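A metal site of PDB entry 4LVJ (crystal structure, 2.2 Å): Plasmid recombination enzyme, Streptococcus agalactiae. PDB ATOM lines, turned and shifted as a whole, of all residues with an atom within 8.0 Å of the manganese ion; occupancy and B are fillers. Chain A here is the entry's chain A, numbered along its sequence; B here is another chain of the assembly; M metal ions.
OE2 of Glu 128 sits close to NH2 of Arg 24, at 2.8 Å. A ring nitrogen (ND1) of His 132 lies within hydrogen-bond range of the backbone carbonyl oxygen (O) of Thr 130, at 2.9 Å. OP1 of DG 15 of chain B sits at hydrogen-bond distance from the backbone NH (N) of Ser 129 (2.8 Å). NE2 of His 125 lies within hydrogen-bond range of O of Asn 22, 3.2 Å away. A ring nitrogen (NE2) of His 125 is in hydrogen-bond range of the side-chain hydroxyl (OG) of Ser 123 (3.1 Å). The backbone carbonyl oxygen of Ser 123 lies within hydrogen-bond range of the backbone NH of His 134, at 2.9 Å. OE1 of Glu 81 sits at hydrogen-bond distance from ND1 of His 134, at 2.9 Å. The backbone carbonyl oxygen of His 21 lies within hydrogen-bond range of the guanidinium group of Arg 24 (2.7 Å).
OE2 of Glu 128 binds the manganese ion, 2.2 Å away. A ring nitrogen (NE2) of His 132 binds the manganese ion. O3' of DG 15 of chain B binds the manganese ion. A ring nitrogen (ND1) of His 125 is bound to the manganese ion, at 2.3 Å. NE2 of His 134 binds the manganese ion (2.3 Å). The manganese ion is bound by a ring nitrogen (NE2) of His 21, 2.5 Å away. The manganese ion has six donor atoms within binding distance.
Six residues have an atom within 4 Å of the manganese ion: His 21, His 125, Glu 128, His 132, His 134 and DG 15 of chain B.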
ATOM      1  N   HIS A  21     -28.930  25.015 -25.047  1.00  0.00           N
ATOM      2  CA  HIS A  21     -28.772  23.720 -24.418  1.00  0.00           C
ATOM      3  C   HIS A  21     -27.741  22.914 -25.231  1.00  0.00           C
ATOM      4  O   HIS A  21     -26.776  22.378 -24.672  1.00  0.00           O
ATOM      5  CB  HIS A  21     -30.129  22.972 -24.292  1.00  0.00           C
ATOM      6  CG  HIS A  21     -29.982  21.494 -23.988  1.00  0.00           C
ATOM      7  ND1 HIS A  21     -29.829  21.006 -22.703  1.00  0.00           N
ATOM      8  CD2 HIS A  21     -29.936  20.414 -24.804  1.00  0.00           C
ATOM      9  CE1 HIS A  21     -29.693  19.686 -22.743  1.00  0.00           C
ATOM     10  NE2 HIS A  21     -29.754  19.309 -24.009  1.00  0.00           N
ATOM     11  N   ASN A  22     -27.958  22.841 -26.544  1.00  0.00           N
ATOM     12  CA  ASN A  22     -27.182  21.937 -27.381  1.00  0.00           C
ATOM     13  C   ASN A  22     -25.699  22.279 -27.391  1.00  0.00           C
ATOM     14  O   ASN A  22     -24.862  21.348 -27.428  1.00  0.00           O
ATOM     15  CB  ASN A  22     -27.715  21.841 -28.812  1.00  0.00           C
ATOM     16  CG  ASN A  22     -29.069  21.154 -28.899  1.00  0.00           C
ATOM     17  OD1 ASN A  22     -29.681  20.765 -27.881  1.00  0.00           O
ATOM     18  ND2 ASN A  22     -29.560  21.025 -30.130  1.00  0.00           N
ATOM     19  N   ARG A  24     -24.102  24.102 -25.027  1.00  0.00           N
ATOM     20  CA  ARG A  24     -23.699  24.349 -23.661  1.00  0.00           C
ATOM     21  C   ARG A  24     -23.205  25.767 -23.394  1.00  0.00           C
ATOM     22  O   ARG A  24     -22.078  25.975 -22.969  1.00  0.00           O
ATOM     23  CB  ARG A  24     -22.703  23.288 -23.218  1.00  0.00           C
ATOM     24  CG  ARG A  24     -23.246  21.884 -23.369  1.00  0.00           C
ATOM     25  CD  ARG A  24     -24.110  21.492 -22.182  1.00  0.00           C
ATOM     26  NE  ARG A  24     -24.447  20.071 -22.204  1.00  0.00           N
ATOM     27  CZ  ARG A  24     -25.642  19.567 -22.545  1.00  0.00           C
ATOM     28  NH1 ARG A  24     -26.620  20.392 -22.892  1.00  0.00           N
ATOM     29  NH2 ARG A  24     -25.850  18.246 -22.530  1.00  0.00           N
ATOM     30  N   ILE A  34     -26.566  17.609 -15.618  1.00  0.00           N
ATOM     31  CA  ILE A  34     -25.486  17.762 -16.598  1.00  0.00           C
ATOM     32  C   ILE A  34     -24.142  17.704 -15.878  1.00  0.00           C
ATOM     33  O   ILE A  34     -23.899  18.524 -15.005  1.00  0.00           O
ATOM     34  CB  ILE A  34     -25.608  19.069 -17.417  1.00  0.00           C
ATOM     35  CG1 ILE A  34     -26.771  18.952 -18.407  1.00  0.00           C
ATOM     36  CG2 ILE A  34     -24.311  19.373 -18.192  1.00  0.00           C
ATOM     37  CD1 ILE A  34     -27.329  20.273 -18.869  1.00  0.00           C
ATOM     38  N   ASN A  42     -18.833  15.839 -25.473  1.00  0.00           N
ATOM     39  CA  ASN A  42     -19.841  15.957 -26.496  1.00  0.00           C
ATOM     40  C   ASN A  42     -19.280  16.198 -27.893  1.00  0.00           C
ATOM     41  O   ASN A  42     -18.148  16.602 -28.016  1.00  0.00           O
ATOM     42  CB  ASN A  42     -20.808  17.060 -26.107  1.00  0.00           C
ATOM     43  CG  ASN A  42     -21.580  16.704 -24.894  1.00  0.00           C
ATOM     44  OD1 ASN A  42     -21.458  15.596 -24.368  1.00  0.00           O
ATOM     45  ND2 ASN A  42     -22.387  17.640 -24.416  1.00  0.00           N
ATOM     46  N   GLU A  81     -36.745  18.766 -34.329  1.00  0.00           N
ATOM     47  CA  GLU A  81     -35.648  18.248 -33.569  1.00  0.00           C
ATOM     48  C   GLU A  81     -36.011  16.850 -33.106  1.00  0.00           C
ATOM     49  O   GLU A  81     -36.878  16.685 -32.250  1.00  0.00           O
ATOM     50  CB  GLU A  81     -35.267  19.168 -32.392  1.00  0.00           C
ATOM     51  CG  GLU A  81     -34.043  18.615 -31.688  1.00  0.00           C
ATOM     52  CD  GLU A  81     -33.600  19.435 -30.507  1.00  0.00           C
ATOM     53  OE1 GLU A  81     -33.980  19.077 -29.362  1.00  0.00           O
ATOM     54  OE2 GLU A  81     -32.874  20.450 -30.736  1.00  0.00           O
ATOM     55  N   ILE A  83     -34.912  13.628 -31.007  1.00  0.00           N
ATOM     56  CA  ILE A  83     -34.098  12.935 -30.016  1.00  0.00           C
ATOM     57  C   ILE A  83     -33.800  11.517 -30.555  1.00  0.00           C
ATOM     58  O   ILE A  83     -34.719  10.819 -31.063  1.00  0.00           O
ATOM     59  CB  ILE A  83     -34.824  12.884 -28.659  1.00  0.00           C
ATOM     60  CG1 ILE A  83     -35.008  14.301 -28.131  1.00  0.00           C
ATOM     61  CG2 ILE A  83     -34.026  12.148 -27.595  1.00  0.00           C
ATOM     62  CD1 ILE A  83     -33.744  15.127 -28.130  1.00  0.00           C
ATOM     63  N   SER A 123     -26.331  17.064 -32.605  1.00  0.00           N
ATOM     64  CA  SER A 123     -25.510  17.373 -31.449  1.00  0.00           C
ATOM     65  C   SER A 123     -25.613  16.192 -30.452  1.00  0.00           C
ATOM     66  O   SER A 123     -26.708  15.878 -29.967  1.00  0.00           O
ATOM     67  CB  SER A 123     -25.983  18.713 -30.879  1.00  0.00           C
ATOM     68  OG  SER A 123     -25.415  18.929 -29.615  1.00  0.00           O
ATOM     69  N   VAL A 124     -24.486  15.564 -30.159  1.00  0.00           N
ATOM     70  CA  VAL A 124     -24.446  14.368 -29.332  1.00  0.00           C
ATOM     71  C   VAL A 124     -23.992  14.689 -27.906  1.00  0.00           C
ATOM     72  O   VAL A 124     -22.883  15.195 -27.687  1.00  0.00           O
ATOM     73  CB  VAL A 124     -23.460  13.318 -29.908  1.00  0.00           C
ATOM     74  CG1 VAL A 124     -23.341  12.130 -28.963  1.00  0.00           C
ATOM     75  CG2 VAL A 124     -23.908  12.867 -31.303  1.00  0.00           C
ATOM     76  N   HIS A 125     -24.850  14.339 -26.944  1.00  0.00           N
ATOM     77  CA  HIS A 125     -24.605  14.631 -25.561  1.00  0.00           C
ATOM     78  C   HIS A 125     -24.277  13.406 -24.760  1.00  0.00           C
ATOM     79  O   HIS A 125     -25.099  12.470 -24.615  1.00  0.00           O
ATOM     80  CB  HIS A 125     -25.796  15.326 -24.928  1.00  0.00           C
ATOM     81  CG  HIS A 125     -26.155  16.626 -25.566  1.00  0.00           C
ATOM     82  ND1 HIS A 125     -27.315  17.297 -25.260  1.00  0.00           N
ATOM     83  CD2 HIS A 125     -25.496  17.390 -26.483  1.00  0.00           C
ATOM     84  CE1 HIS A 125     -27.342  18.441 -25.925  1.00  0.00           C
ATOM     85  NE2 HIS A 125     -26.257  18.522 -26.688  1.00  0.00           N
ATOM     86  N   LEU A 126     -23.072  13.436 -24.197  1.00  0.00           N
ATOM     87  CA  LEU A 126     -22.596  12.346 -23.340  1.00  0.00           C
ATOM     88  C   LEU A 126     -22.467  12.835 -21.892  1.00  0.00           C
ATOM     89  O   LEU A 126     -22.067  12.070 -21.027  1.00  0.00           O
ATOM     90  CB  LEU A 126     -21.276  11.751 -23.871  1.00  0.00           C
ATOM     91  CG  LEU A 126     -21.288  11.351 -25.371  1.00  0.00           C
ATOM     92  CD1 LEU A 126     -19.948  10.764 -25.793  1.00  0.00           C
ATOM     93  CD2 LEU A 126     -22.403  10.396 -25.701  1.00  0.00           C
ATOM     94  N   ASP A 127     -22.813  14.097 -21.640  1.00  0.00           N
ATOM     95  CA  ASP A 127     -22.633  14.651 -20.299  1.00  0.00           C
ATOM     96  C   ASP A 127     -23.920  14.682 -19.458  1.00  0.00           C
ATOM     97  O   ASP A 127     -23.941  15.258 -18.383  1.00  0.00           O
ATOM     98  CB  ASP A 127     -21.993  16.029 -20.395  1.00  0.00           C
ATOM     99  CG  ASP A 127     -22.822  17.039 -21.213  1.00  0.00           C
ATOM    100  OD1 ASP A 127     -23.704  16.651 -22.024  1.00  0.00           O
ATOM    101  OD2 ASP A 127     -22.525  18.244 -21.049  1.00  0.00           O
ATOM    102  N   GLU A 128     -24.975  14.026 -19.944  1.00  0.00           N
ATOM    103  CA  GLU A 128     -26.218  13.850 -19.178  1.00  0.00           C
ATOM    104  C   GLU A 128     -26.334  12.366 -18.792  1.00  0.00           C
ATOM    105  O   GLU A 128     -25.314  11.665 -18.800  1.00  0.00           O
ATOM    106  CB  GLU A 128     -27.445  14.388 -19.964  1.00  0.00           C
ATOM    107  CG  GLU A 128     -27.339  15.878 -20.319  1.00  0.00           C
ATOM    108  CD  GLU A 128     -28.478  16.356 -21.221  1.00  0.00           C
ATOM    109  OE1 GLU A 128     -29.631  16.357 -20.739  1.00  0.00           O
ATOM    110  OE2 GLU A 128     -28.235  16.734 -22.386  1.00  0.00           O
ATOM    111  N   SER A 129     -27.535  11.879 -18.462  1.00  0.00           N
ATOM    112  CA  SER A 129     -27.690  10.507 -17.941  1.00  0.00           C
ATOM    113  C   SER A 129     -27.327   9.411 -18.914  1.00  0.00           C
ATOM    114  O   SER A 129     -26.715   8.434 -18.518  1.00  0.00           O
ATOM    115  CB  SER A 129     -29.106  10.236 -17.481  1.00  0.00           C
ATOM    116  OG  SER A 129     -29.366  10.916 -16.268  1.00  0.00           O
ATOM    117  N   THR A 130     -27.751   9.565 -20.168  1.00  0.00           N
ATOM    118  CA  THR A 130     -27.640   8.542 -21.211  1.00  0.00           C
ATOM    119  C   THR A 130     -27.189   9.262 -22.472  1.00  0.00           C
ATOM    120  O   THR A 130     -27.611  10.391 -22.710  1.00  0.00           O
ATOM    121  CB  THR A 130     -29.007   7.872 -21.488  1.00  0.00           C
ATOM    122  OG1 THR A 130     -29.646   7.525 -20.243  1.00  0.00           O
ATOM    123  CG2 THR A 130     -28.868   6.604 -22.337  1.00  0.00           C
ATOM    124  N   PRO A 131     -26.346   8.616 -23.307  1.00  0.00           N
ATOM    125  CA  PRO A 131     -26.020   9.204 -24.604  1.00  0.00           C
ATOM    126  C   PRO A 131     -27.282   9.427 -25.437  1.00  0.00           C
ATOM    127  O   PRO A 131     -28.170   8.520 -25.511  1.00  0.00           O
ATOM    128  CB  PRO A 131     -25.157   8.104 -25.272  1.00  0.00           C
ATOM    129  CG  PRO A 131     -24.587   7.336 -24.113  1.00  0.00           C
ATOM    130  CD  PRO A 131     -25.602   7.372 -23.036  1.00  0.00           C
ATOM    131  N   HIS A 132     -27.363  10.607 -26.039  1.00  0.00           N
ATOM    132  CA  HIS A 132     -28.451  10.970 -26.961  1.00  0.00           C
ATOM    133  C   HIS A 132     -28.005  12.058 -27.945  1.00  0.00           C
ATOM    134  O   HIS A 132     -26.991  12.746 -27.709  1.00  0.00           O
ATOM    135  CB  HIS A 132     -29.675  11.435 -26.183  1.00  0.00           C
ATOM    136  CG  HIS A 132     -29.434  12.650 -25.339  1.00  0.00           C
ATOM    137  ND1 HIS A 132     -28.769  12.598 -24.124  1.00  0.00           N
ATOM    138  CD2 HIS A 132     -29.776  13.954 -25.521  1.00  0.00           C
ATOM    139  CE1 HIS A 132     -28.722  13.813 -23.594  1.00  0.00           C
ATOM    140  NE2 HIS A 132     -29.331  14.655 -24.415  1.00  0.00           N
ATOM    141  N   MET A 133     -28.778  12.229 -29.016  1.00  0.00           N
ATOM    142  CA  MET A 133     -28.452  13.188 -30.057  1.00  0.00           C
ATOM    143  C   MET A 133     -29.680  14.043 -30.244  1.00  0.00           C
ATOM    144  O   MET A 133     -30.795  13.471 -30.330  1.00  0.00           O
ATOM    145  CB  MET A 133     -28.129  12.470 -31.378  1.00  0.00           C
ATOM    146  CG  MET A 133     -27.673  13.401 -32.510  1.00  0.00           C
ATOM    147  SD  MET A 133     -27.143  12.481 -33.979  1.00  0.00           S
ATOM    148  CE  MET A 133     -28.595  11.490 -34.342  1.00  0.00           C
ATOM    149  N   HIS A 134     -29.501  15.381 -30.281  1.00  0.00           N
ATOM    150  CA  HIS A 134     -30.580  16.294 -30.703  1.00  0.00           C
ATOM    151  C   HIS A 134     -30.286  16.565 -32.147  1.00  0.00           C
ATOM    152  O   HIS A 134     -29.255  17.167 -32.438  1.00  0.00           O
ATOM    153  CB  HIS A 134     -30.523  17.629 -29.946  1.00  0.00           C
ATOM    154  CG  HIS A 134     -30.669  17.506 -28.457  1.00  0.00           C
ATOM    155  ND1 HIS A 134     -31.823  17.871 -27.786  1.00  0.00           N
ATOM    156  CD2 HIS A 134     -29.810  17.042 -27.511  1.00  0.00           C
ATOM    157  CE1 HIS A 134     -31.650  17.644 -26.486  1.00  0.00           C
ATOM    158  NE2 HIS A 134     -30.428  17.169 -26.295  1.00  0.00           N
ATOM    159  N   VAL A 188     -39.187  16.009 -20.127  1.00  0.00           N
ATOM    160  CA  VAL A 188     -38.026  15.577 -19.320  1.00  0.00           C
ATOM    161  C   VAL A 188     -38.256  15.829 -17.812  1.00  0.00           C
ATOM    162  O   VAL A 188     -38.020  14.933 -16.964  1.00  0.00           O
ATOM    163  CB  VAL A 188     -36.703  16.241 -19.793  1.00  0.00           C
ATOM    164  CG1 VAL A 188     -35.604  16.069 -18.753  1.00  0.00           C
ATOM    165  CG2 VAL A 188     -36.264  15.634 -21.124  1.00  0.00           C
ATOM    166  P    DG B  15     -31.430  13.700 -18.383  1.00  0.00           P
ATOM    167  OP1  DG B  15     -30.131  13.017 -18.277  1.00  0.00           O
ATOM    168  OP2  DG B  15     -31.526  15.090 -17.876  1.00  0.00           O
ATOM    169  O5'  DG B  15     -31.913  13.635 -19.899  1.00  0.00           O
ATOM    170  C5'  DG B  15     -32.518  14.751 -20.601  1.00  0.00           C
ATOM    171  C4'  DG B  15     -32.223  14.629 -22.082  1.00  0.00           C
ATOM    172  O4'  DG B  15     -33.099  13.632 -22.661  1.00  0.00           O
ATOM    173  C3'  DG B  15     -32.437  15.889 -22.916  1.00  0.00           C
ATOM    174  O3'  DG B  15     -31.189  16.548 -23.049  1.00  0.00           O
ATOM    175  C2'  DG B  15     -32.869  15.373 -24.304  1.00  0.00           C
ATOM    176  C1'  DG B  15     -33.349  13.940 -24.017  1.00  0.00           C
ATOM    177  N9   DG B  15     -34.770  13.685 -24.285  1.00  0.00           N
ATOM    178  C8   DG B  15     -35.753  14.600 -24.563  1.00  0.00           C
ATOM    179  N7   DG B  15     -36.934  14.066 -24.701  1.00  0.00           N
ATOM    180  C5   DG B  15     -36.718  12.704 -24.511  1.00  0.00           C
ATOM    181  C6   DG B  15     -37.624  11.614 -24.527  1.00  0.00           C
ATOM    182  O6   DG B  15     -38.854  11.631 -24.730  1.00  0.00           O
ATOM    183  N1   DG B  15     -36.978  10.403 -24.268  1.00  0.00           N
ATOM    184  C2   DG B  15     -35.639  10.261 -24.014  1.00  0.00           C
ATOM    185  N2   DG B  15     -35.208   9.008 -23.780  1.00  0.00           N
ATOM    186  N3   DG B  15     -34.789  11.271 -23.973  1.00  0.00           N
ATOM    187  C4   DG B  15     -35.393  12.455 -24.226  1.00  0.00           C
HETATM  188 MN    MN M   1     -29.342  16.862 -24.267  1.00  0.00          MN
